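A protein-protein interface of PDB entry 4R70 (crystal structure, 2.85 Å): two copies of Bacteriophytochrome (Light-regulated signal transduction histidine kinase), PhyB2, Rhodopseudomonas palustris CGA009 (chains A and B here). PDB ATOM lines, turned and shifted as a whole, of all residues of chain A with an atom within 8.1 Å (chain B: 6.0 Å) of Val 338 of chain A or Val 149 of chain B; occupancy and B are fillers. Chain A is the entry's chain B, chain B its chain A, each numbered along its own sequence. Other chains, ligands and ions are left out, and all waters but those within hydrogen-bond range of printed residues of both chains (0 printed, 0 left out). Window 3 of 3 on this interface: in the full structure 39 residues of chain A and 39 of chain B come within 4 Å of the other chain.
The backbone carbonyl oxygen (O) of Val 334 of chain A is in hydrogen-bond range of the side-chain hydroxyl (OG) of Ser 337 of chain A (2.5 Å).
Among the printed residues, pairs that only touch across the chains: Arg 335 of chain A with Arg 150 of chain B (3.1 Å), Arg 335 of chain A with Arg 154 of chain B (3.7 Å), His 336 of chain A with Arg 150 of chain B (3.4 Å), Ser 337 of chain A with Leu 316 of chain B (3.4 Å), Val 338 of chain A with Val 149 of chain B (3.3 Å), Val 338 of chain A with Leu 316 of chain B (3.4 Å), Arg 339 of chain A with Phe 146 of chain B (3.2 Å) and Ala 342 of chain A with Phe 146 of chain B (3.6 Å).
Of the 15 printed residues of chain B, 5 touch a printed residue of chain A. Printed residues of chain B that touch a printed residue of chain A: Phe 146, Val 149, Arg 150, Arg 154 and Leu 316. Hydrophobic or aromatic side chains of chain B that line the printed part of chain A: Phe 146, Val 149 and Leu 316. Printed residues of chain A that touch a printed residue of chain B: Arg 335, His 336, Ser 337, Val 338, Arg 339 and Ala 342. Hydrophobic or aromatic side chains of chain A within 4 Å of the printed part of chain B: His 336, Val 338 and Ala 342. Among the printed residues, 8 pairs touch across the chains. Among the printed residues, no Asp or Glu carboxylate lies within 4 Å of a Lys or Arg side-chain nitrogen of the other chain.
No position is printed for both chains.
Printed residues of chain B within 4 Å of Val 338 of chain A: Val 149 and Leu 316. Val 149 of chain B touches just one residue of chain A: Val 338 (3.3 Å). No residue of chain A comes within 4 Å of Ser 148 of chain B. Printed residues of chain B within 4 Å of Ala 342 of chain A: Phe 146. Printed residues of chain B within 4 Å of His 336 of chain A: Arg 150. Printed residues of chain A within 4 Å of Phe 146 of chain B: Arg 339 (3.2 Å) and Ala 342 (3.6 Å). Gln 344 of chain A touches none of the printed residues of chain B. The nearest printed residue of chain A that does not touch Leu 316 of chain B is Arg 341 of chain A (5.0 Å).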
ATOM      1  N   ILE A 333      15.713 -27.331   6.100  1.00  0.00           N
ATOM      2  CA  ILE A 333      14.756 -26.924   5.160  1.00  0.00           C
ATOM      3  C   ILE A 333      13.472 -27.751   5.228  1.00  0.00           C
ATOM      4  O   ILE A 333      12.363 -27.251   5.100  1.00  0.00           O
ATOM      5  CB  ILE A 333      15.320 -27.092   3.787  1.00  0.00           C
ATOM      6  CG1 ILE A 333      16.302 -25.960   3.467  1.00  0.00           C
ATOM      7  CG2 ILE A 333      14.288 -26.985   2.778  1.00  0.00           C
ATOM      8  CD1 ILE A 333      17.284 -26.283   2.478  1.00  0.00           C
ATOM      9  N   VAL A 334      13.591 -29.042   5.376  1.00  0.00           N
ATOM     10  CA  VAL A 334      12.390 -29.838   5.364  1.00  0.00           C
ATOM     11  C   VAL A 334      11.442 -29.503   6.497  1.00  0.00           C
ATOM     12  O   VAL A 334      10.205 -29.469   6.293  1.00  0.00           O
ATOM     13  CB  VAL A 334      12.766 -31.286   5.426  1.00  0.00           C
ATOM     14  CG1 VAL A 334      11.559 -32.195   5.635  1.00  0.00           C
ATOM     15  CG2 VAL A 334      13.409 -31.585   4.178  1.00  0.00           C
ATOM     16  N   ARG A 335      12.032 -29.241   7.665  1.00  0.00           N
ATOM     17  CA  ARG A 335      11.316 -29.008   8.904  1.00  0.00           C
ATOM     18  C   ARG A 335      10.329 -27.896   8.735  1.00  0.00           C
ATOM     19  O   ARG A 335       9.317 -27.799   9.430  1.00  0.00           O
ATOM     20  CB  ARG A 335      12.293 -28.586   9.954  1.00  0.00           C
ATOM     21  CG  ARG A 335      13.009 -29.651  10.600  1.00  0.00           C
ATOM     22  CD  ARG A 335      13.580 -29.189  11.910  1.00  0.00           C
ATOM     23  NE  ARG A 335      15.016 -28.936  11.827  1.00  0.00           N
ATOM     24  CZ  ARG A 335      15.859 -29.940  11.819  1.00  0.00           C
ATOM     25  NH1 ARG A 335      15.356 -31.143  11.843  1.00  0.00           N
ATOM     26  NH2 ARG A 335      17.167 -29.770  11.743  1.00  0.00           N
ATOM     27  N   HIS A 336      10.564 -27.126   7.698  1.00  0.00           N
ATOM     28  CA  HIS A 336       9.908 -25.883   7.492  1.00  0.00           C
ATOM     29  C   HIS A 336       9.073 -25.874   6.192  1.00  0.00           C
ATOM     30  O   HIS A 336       8.493 -24.875   5.815  1.00  0.00           O
ATOM     31  CB  HIS A 336      11.028 -24.818   7.489  1.00  0.00           C
ATOM     32  CG  HIS A 336      11.671 -24.578   8.847  1.00  0.00           C
ATOM     33  ND1 HIS A 336      13.026 -24.422   9.007  1.00  0.00           N
ATOM     34  CD2 HIS A 336      11.120 -24.373  10.076  1.00  0.00           C
ATOM     35  CE1 HIS A 336      13.302 -24.185  10.280  1.00  0.00           C
ATOM     36  NE2 HIS A 336      12.157 -24.137  10.946  1.00  0.00           N
ATOM     37  N   SER A 337       8.944 -27.021   5.544  1.00  0.00           N
ATOM     38  CA  SER A 337       8.131 -27.139   4.333  1.00  0.00           C
ATOM     39  C   SER A 337       6.674 -26.935   4.609  1.00  0.00           C
ATOM     40  O   SER A 337       5.862 -26.809   3.691  1.00  0.00           O
ATOM     41  CB  SER A 337       8.273 -28.525   3.743  1.00  0.00           C
ATOM     42  OG  SER A 337       8.177 -29.464   4.785  1.00  0.00           O
ATOM     43  N   VAL A 338       6.337 -26.989   5.889  1.00  0.00           N
ATOM     44  CA  VAL A 338       4.955 -27.063   6.261  1.00  0.00           C
ATOM     45  C   VAL A 338       4.223 -25.743   6.181  1.00  0.00           C
ATOM     46  O   VAL A 338       3.232 -25.660   5.449  1.00  0.00           O
ATOM     47  CB  VAL A 338       4.811 -27.689   7.575  1.00  0.00           C
ATOM     48  CG1 VAL A 338       4.408 -29.087   7.305  1.00  0.00           C
ATOM     49  CG2 VAL A 338       6.182 -27.565   8.376  1.00  0.00           C
ATOM     50  N   ARG A 339       4.682 -24.725   6.919  1.00  0.00           N
ATOM     51  CA  ARG A 339       4.135 -23.364   6.772  1.00  0.00           C
ATOM     52  C   ARG A 339       4.110 -23.050   5.300  1.00  0.00           C
ATOM     53  O   ARG A 339       3.171 -22.501   4.709  1.00  0.00           O
ATOM     54  CB  ARG A 339       5.007 -22.336   7.469  1.00  0.00           C
ATOM     55  CG  ARG A 339       4.975 -22.506   8.918  1.00  0.00           C
ATOM     56  CD  ARG A 339       4.836 -21.217   9.629  1.00  0.00           C
ATOM     57  NE  ARG A 339       6.132 -20.605   9.774  1.00  0.00           N
ATOM     58  CZ  ARG A 339       6.288 -19.372  10.205  1.00  0.00           C
ATOM     59  NH1 ARG A 339       5.206 -18.663  10.523  1.00  0.00           N
ATOM     60  NH2 ARG A 339       7.518 -18.872  10.329  1.00  0.00           N
ATOM     61  N   MET A 340       5.207 -23.462   4.722  1.00  0.00           N
ATOM     62  CA  MET A 340       5.530 -23.154   3.396  1.00  0.00           C
ATOM     63  C   MET A 340       4.418 -23.677   2.508  1.00  0.00           C
ATOM     64  O   MET A 340       3.824 -22.924   1.767  1.00  0.00           O
ATOM     65  CB  MET A 340       6.861 -23.797   3.112  1.00  0.00           C
ATOM     66  CG  MET A 340       7.932 -22.777   2.794  1.00  0.00           C
ATOM     67  SD  MET A 340       7.290 -21.565   1.634  1.00  0.00           S
ATOM     68  CE  MET A 340       6.999 -22.681   0.259  1.00  0.00           C
ATOM     69  N   ARG A 341       4.154 -24.971   2.549  1.00  0.00           N
ATOM     70  CA  ARG A 341       3.001 -25.495   1.807  1.00  0.00           C
ATOM     71  C   ARG A 341       1.716 -24.667   2.092  1.00  0.00           C
ATOM     72  O   ARG A 341       1.083 -24.104   1.185  1.00  0.00           O
ATOM     73  CB  ARG A 341       2.779 -26.972   2.153  1.00  0.00           C
ATOM     74  CG  ARG A 341       2.738 -27.961   0.989  1.00  0.00           C
ATOM     75  CD  ARG A 341       1.372 -27.887   0.259  1.00  0.00           C
ATOM     76  NE  ARG A 341       1.346 -28.766  -0.904  1.00  0.00           N
ATOM     77  CZ  ARG A 341       2.100 -28.599  -1.988  1.00  0.00           C
ATOM     78  NH1 ARG A 341       2.948 -27.576  -2.080  1.00  0.00           N
ATOM     79  NH2 ARG A 341       2.001 -29.460  -2.995  1.00  0.00           N
ATOM     80  N   ALA A 342       1.419 -24.520   3.381  1.00  0.00           N
ATOM     81  CA  ALA A 342       0.264 -23.777   3.822  1.00  0.00           C
ATOM     82  C   ALA A 342       0.253 -22.359   3.265  1.00  0.00           C
ATOM     83  O   ALA A 342      -0.745 -21.889   2.700  1.00  0.00           O
ATOM     84  CB  ALA A 342       0.287 -23.698   5.318  1.00  0.00           C
ATOM     85  N   ILE A 343       1.357 -21.667   3.482  1.00  0.00           N
ATOM     86  CA  ILE A 343       1.485 -20.299   3.036  1.00  0.00           C
ATOM     87  C   ILE A 343       1.331 -20.178   1.487  1.00  0.00           C
ATOM     88  O   ILE A 343       0.600 -19.313   0.993  1.00  0.00           O
ATOM     89  CB  ILE A 343       2.723 -19.672   3.713  1.00  0.00           C
ATOM     90  CG1 ILE A 343       2.278 -19.153   5.089  1.00  0.00           C
ATOM     91  CG2 ILE A 343       3.381 -18.628   2.883  1.00  0.00           C
ATOM     92  CD1 ILE A 343       3.411 -18.723   5.997  1.00  0.00           C
ATOM     93  N   GLN A 344       1.910 -21.124   0.752  1.00  0.00           N
ATOM     94  CA  GLN A 344       1.759 -21.137  -0.687  1.00  0.00           C
ATOM     95  C   GLN A 344       0.286 -21.107  -1.018  1.00  0.00           C
ATOM     96  O   GLN A 344      -0.190 -20.345  -1.875  1.00  0.00           O
ATOM     97  CB  GLN A 344       2.398 -22.389  -1.332  1.00  0.00           C
ATOM     98  CG  GLN A 344       3.952 -22.504  -1.246  1.00  0.00           C
ATOM     99  CD  GLN A 344       4.544 -23.733  -1.993  1.00  0.00           C
ATOM    100  OE1 GLN A 344       3.893 -24.771  -2.105  1.00  0.00           O
ATOM    101  NE2 GLN A 344       5.800 -23.622  -2.454  1.00  0.00           N
ATOM    102  N   ASN A 345      -0.409 -22.017  -0.357  1.00  0.00           N
ATOM    103  CA  ASN A 345      -1.814 -22.210  -0.584  1.00  0.00           C
ATOM    104  C   ASN A 345      -2.573 -20.919  -0.374  1.00  0.00           C
ATOM    105  O   ASN A 345      -3.368 -20.499  -1.217  1.00  0.00           O
ATOM    106  CB  ASN A 345      -2.357 -23.307   0.296  1.00  0.00           C
ATOM    107  CG  ASN A 345      -3.679 -23.793  -0.187  1.00  0.00           C
ATOM    108  OD1 ASN A 345      -4.733 -23.300   0.228  1.00  0.00           O
ATOM    109  ND2 ASN A 345      -3.638 -24.699  -1.183  1.00  0.00           N
ATOM    110  N   LEU A 371       7.844 -15.593   8.313  1.00  0.00           N
ATOM    111  CA  LEU A 371       8.474 -16.816   7.927  1.00  0.00           C
ATOM    112  C   LEU A 371       9.980 -16.513   7.803  1.00  0.00           C
ATOM    113  O   LEU A 371      10.802 -17.138   8.480  1.00  0.00           O
ATOM    114  CB  LEU A 371       7.833 -17.264   6.643  1.00  0.00           C
ATOM    115  CG  LEU A 371       8.006 -18.731   6.285  1.00  0.00           C
ATOM    116  CD1 LEU A 371       7.623 -18.878   4.809  1.00  0.00           C
ATOM    117  CD2 LEU A 371       9.444 -19.287   6.567  1.00  0.00           C
ATOM    118  N   GLU B 144       0.336 -23.263  16.220  1.00  0.00           N
ATOM    119  CA  GLU B 144       0.645 -24.414  17.078  1.00  0.00           C
ATOM    120  C   GLU B 144       0.788 -25.659  16.246  1.00  0.00           C
ATOM    121  O   GLU B 144       1.585 -26.535  16.506  1.00  0.00           O
ATOM    122  CB  GLU B 144      -0.351 -24.585  18.238  1.00  0.00           C
ATOM    123  CG  GLU B 144      -0.255 -25.903  19.073  1.00  0.00           C
ATOM    124  CD  GLU B 144      -1.168 -27.041  18.498  1.00  0.00           C
ATOM    125  OE1 GLU B 144      -0.816 -28.243  18.662  1.00  0.00           O
ATOM    126  OE2 GLU B 144      -2.198 -26.721  17.824  1.00  0.00           O
ATOM    127  N   PHE B 145       0.048 -25.726  15.181  1.00  0.00           N
ATOM    128  CA  PHE B 145       0.084 -26.923  14.380  1.00  0.00           C
ATOM    129  C   PHE B 145       1.434 -27.003  13.681  1.00  0.00           C
ATOM    130  O   PHE B 145       2.058 -28.064  13.655  1.00  0.00           O
ATOM    131  CB  PHE B 145      -1.034 -26.824  13.386  1.00  0.00           C
ATOM    132  CG  PHE B 145      -1.112 -27.937  12.440  1.00  0.00           C
ATOM    133  CD1 PHE B 145      -1.910 -29.034  12.723  1.00  0.00           C
ATOM    134  CD2 PHE B 145      -0.488 -27.870  11.220  1.00  0.00           C
ATOM    135  CE1 PHE B 145      -2.053 -30.068  11.850  1.00  0.00           C
ATOM    136  CE2 PHE B 145      -0.638 -28.901  10.361  1.00  0.00           C
ATOM    137  CZ  PHE B 145      -1.441 -30.001  10.689  1.00  0.00           C
ATOM    138  N   PHE B 146       1.859 -25.895  13.086  1.00  0.00           N
ATOM    139  CA  PHE B 146       3.122 -25.870  12.391  1.00  0.00           C
ATOM    140  C   PHE B 146       4.245 -26.384  13.212  1.00  0.00           C
ATOM    141  O   PHE B 146       5.069 -27.150  12.725  1.00  0.00           O
ATOM    142  CB  PHE B 146       3.445 -24.497  11.811  1.00  0.00           C
ATOM    143  CG  PHE B 146       2.495 -24.097  10.767  1.00  0.00           C
ATOM    144  CD1 PHE B 146       1.848 -25.092  10.053  1.00  0.00           C
ATOM    145  CD2 PHE B 146       2.156 -22.783  10.553  1.00  0.00           C
ATOM    146  CE1 PHE B 146       0.903 -24.801   9.115  1.00  0.00           C
ATOM    147  CE2 PHE B 146       1.217 -22.457   9.595  1.00  0.00           C
ATOM    148  CZ  PHE B 146       0.568 -23.478   8.874  1.00  0.00           C
ATOM    149  N   ARG B 147       4.296 -25.963  14.470  1.00  0.00           N
ATOM    150  CA  ARG B 147       5.341 -26.450  15.355  1.00  0.00           C
ATOM    151  C   ARG B 147       5.161 -27.944  15.615  1.00  0.00           C
ATOM    152  O   ARG B 147       6.143 -28.676  15.684  1.00  0.00           O
ATOM    153  CB  ARG B 147       5.323 -25.675  16.656  1.00  0.00           C
ATOM    154  CG  ARG B 147       6.237 -24.495  16.662  1.00  0.00           C
ATOM    155  CD  ARG B 147       6.114 -23.779  17.985  1.00  0.00           C
ATOM    156  NE  ARG B 147       5.464 -22.449  17.867  1.00  0.00           N
ATOM    157  CZ  ARG B 147       4.159 -22.220  17.657  1.00  0.00           C
ATOM    158  NH1 ARG B 147       3.322 -23.222  17.519  1.00  0.00           N
ATOM    159  NH2 ARG B 147       3.685 -20.976  17.560  1.00  0.00           N
ATOM    160  N   SER B 148       3.922 -28.417  15.691  1.00  0.00           N
ATOM    161  CA  SER B 148       3.753 -29.820  15.968  1.00  0.00           C
ATOM    162  C   SER B 148       4.345 -30.605  14.803  1.00  0.00           C
ATOM    163  O   SER B 148       5.186 -31.447  15.029  1.00  0.00           O
ATOM    164  CB  SER B 148       2.275 -30.180  16.234  1.00  0.00           C
ATOM    165  OG  SER B 148       1.790 -31.170  15.346  1.00  0.00           O
ATOM    166  N   VAL B 149       4.050 -30.276  13.572  1.00  0.00           N
ATOM    167  CA  VAL B 149       4.712 -31.080  12.560  1.00  0.00           C
ATOM    168  C   VAL B 149       6.235 -30.802  12.541  1.00  0.00           C
ATOM    169  O   VAL B 149       7.018 -31.663  12.182  1.00  0.00           O
ATOM    170  CB  VAL B 149       4.107 -30.984  11.137  1.00  0.00           C
ATOM    171  CG1 VAL B 149       2.633 -30.977  11.209  1.00  0.00           C
ATOM    172  CG2 VAL B 149       4.530 -29.718  10.553  1.00  0.00           C
ATOM    173  N   ARG B 150       6.652 -29.593  12.860  1.00  0.00           N
ATOM    174  CA  ARG B 150       8.085 -29.324  12.832  1.00  0.00           C
ATOM    175  C   ARG B 150       8.727 -30.255  13.806  1.00  0.00           C
ATOM    176  O   ARG B 150       9.700 -30.902  13.456  1.00  0.00           O
ATOM    177  CB  ARG B 150       8.418 -27.886  13.151  1.00  0.00           C
ATOM    178  CG  ARG B 150       9.682 -27.346  12.514  1.00  0.00           C
ATOM    179  CD  ARG B 150       9.888 -25.856  12.874  1.00  0.00           C
ATOM    180  NE  ARG B 150       8.657 -25.094  12.588  1.00  0.00           N
ATOM    181  CZ  ARG B 150       8.051 -24.276  13.454  1.00  0.00           C
ATOM    182  NH1 ARG B 150       6.906 -23.655  13.130  1.00  0.00           N
ATOM    183  NH2 ARG B 150       8.618 -24.047  14.630  1.00  0.00           N
ATOM    184  N   VAL B 151       8.230 -30.326  15.039  1.00  0.00           N
ATOM    185  CA  VAL B 151       8.926 -31.230  15.926  1.00  0.00           C
ATOM    186  C   VAL B 151       8.697 -32.692  15.547  1.00  0.00           C
ATOM    187  O   VAL B 151       9.557 -33.506  15.778  1.00  0.00           O
ATOM    188  CB  VAL B 151       8.700 -31.001  17.428  1.00  0.00           C
ATOM    189  CG1 VAL B 151       8.403 -29.563  17.692  1.00  0.00           C
ATOM    190  CG2 VAL B 151       7.649 -31.857  17.921  1.00  0.00           C
ATOM    191  N   ALA B 152       7.570 -33.039  14.949  1.00  0.00           N
ATOM    192  CA  ALA B 152       7.476 -34.385  14.436  1.00  0.00           C
ATOM    193  C   ALA B 152       8.647 -34.641  13.498  1.00  0.00           C
ATOM    194  O   ALA B 152       9.271 -35.676  13.537  1.00  0.00           O
ATOM    195  CB  ALA B 152       6.171 -34.607  13.710  1.00  0.00           C
ATOM    196  N   ILE B 153       8.914 -33.720  12.614  1.00  0.00           N
ATOM    197  CA  ILE B 153       9.911 -33.991  11.670  1.00  0.00           C
ATOM    198  C   ILE B 153      11.294 -34.069  12.275  1.00  0.00           C
ATOM    199  O   ILE B 153      12.071 -34.890  11.906  1.00  0.00           O
ATOM    200  CB  ILE B 153       9.864 -33.003  10.590  1.00  0.00           C
ATOM    201  CG1 ILE B 153       8.556 -33.154   9.876  1.00  0.00           C
ATOM    202  CG2 ILE B 153      10.940 -33.232   9.628  1.00  0.00           C
ATOM    203  CD1 ILE B 153       8.449 -32.234   8.722  1.00  0.00           C
ATOM    204  N   ARG B 154      11.600 -33.162  13.175  1.00  0.00           N
ATOM    205  CA  ARG B 154      12.901 -33.145  13.782  1.00  0.00           C
ATOM    206  C   ARG B 154      13.110 -34.512  14.377  1.00  0.00           C
ATOM    207  O   ARG B 154      14.135 -35.123  14.156  1.00  0.00           O
ATOM    208  CB  ARG B 154      13.065 -32.007  14.792  1.00  0.00           C
ATOM    209  CG  ARG B 154      14.431 -31.881  15.383  1.00  0.00           C
ATOM    210  CD  ARG B 154      14.477 -30.807  16.474  1.00  0.00           C
ATOM    211  NE  ARG B 154      13.401 -31.031  17.447  1.00  0.00           N
ATOM    212  CZ  ARG B 154      13.010 -30.160  18.375  1.00  0.00           C
ATOM    213  NH1 ARG B 154      13.611 -28.980  18.498  1.00  0.00           N
ATOM    214  NH2 ARG B 154      12.016 -30.471  19.198  1.00  0.00           N
ATOM    215  N   ILE B 176      -1.405 -36.253  15.535  1.00  0.00           N
ATOM    216  CA  ILE B 176      -2.264 -35.293  14.847  1.00  0.00           C
ATOM    217  C   ILE B 176      -3.525 -35.816  14.227  1.00  0.00           C
ATOM    218  O   ILE B 176      -4.405 -35.033  13.981  1.00  0.00           O
ATOM    219  CB  ILE B 176      -1.554 -34.412  13.792  1.00  0.00           C
ATOM    220  CG1 ILE B 176      -1.277 -35.174  12.530  1.00  0.00           C
ATOM    221  CG2 ILE B 176      -0.298 -33.845  14.326  1.00  0.00           C
ATOM    222  CD1 ILE B 176      -0.888 -34.228  11.416  1.00  0.00           C
ATOM    223  N   ALA B 313      -0.440 -33.356   6.008  1.00  0.00           N
ATOM    224  CA  ALA B 313       0.763 -33.432   6.827  1.00  0.00           C
ATOM    225  C   ALA B 313       1.207 -34.877   7.021  1.00  0.00           C
ATOM    226  O   ALA B 313       2.381 -35.149   7.251  1.00  0.00           O
ATOM    227  CB  ALA B 313       0.599 -32.779   8.111  1.00  0.00           C
ATOM    228  N   LEU B 316       3.165 -35.761   4.461  1.00  0.00           N
ATOM    229  CA  LEU B 316       4.423 -35.124   4.580  1.00  0.00           C
ATOM    230  C   LEU B 316       5.296 -35.945   5.514  1.00  0.00           C
ATOM    231  O   LEU B 316       6.421 -36.158   5.241  1.00  0.00           O
ATOM    232  CB  LEU B 316       4.275 -33.699   5.082  1.00  0.00           C
ATOM    233  CG  LEU B 316       5.237 -32.719   4.389  1.00  0.00           C
ATOM    234  CD1 LEU B 316       4.664 -32.124   3.017  1.00  0.00           C
ATOM    235  CD2 LEU B 316       5.719 -31.674   5.450  1.00  0.00           C
ATOM    236  N   ILE B 317       4.760 -36.415   6.601  1.00  0.00           N
ATOM    237  CA  ILE B 317       5.521 -37.285   7.440  1.00  0.00           C
ATOM    238  C   ILE B 317       6.010 -38.510   6.651  1.00  0.00           C
ATOM    239  O   ILE B 317       7.111 -38.939   6.794  1.00  0.00           O
ATOM    240  CB  ILE B 317       4.723 -37.611   8.731  1.00  0.00           C
ATOM    241  CG1 ILE B 317       4.812 -36.381   9.597  1.00  0.00           C
ATOM    242  CG2 ILE B 317       5.307 -38.727   9.494  1.00  0.00           C
ATOM    243  CD1 ILE B 317       3.610 -36.086  10.340  1.00  0.00           C
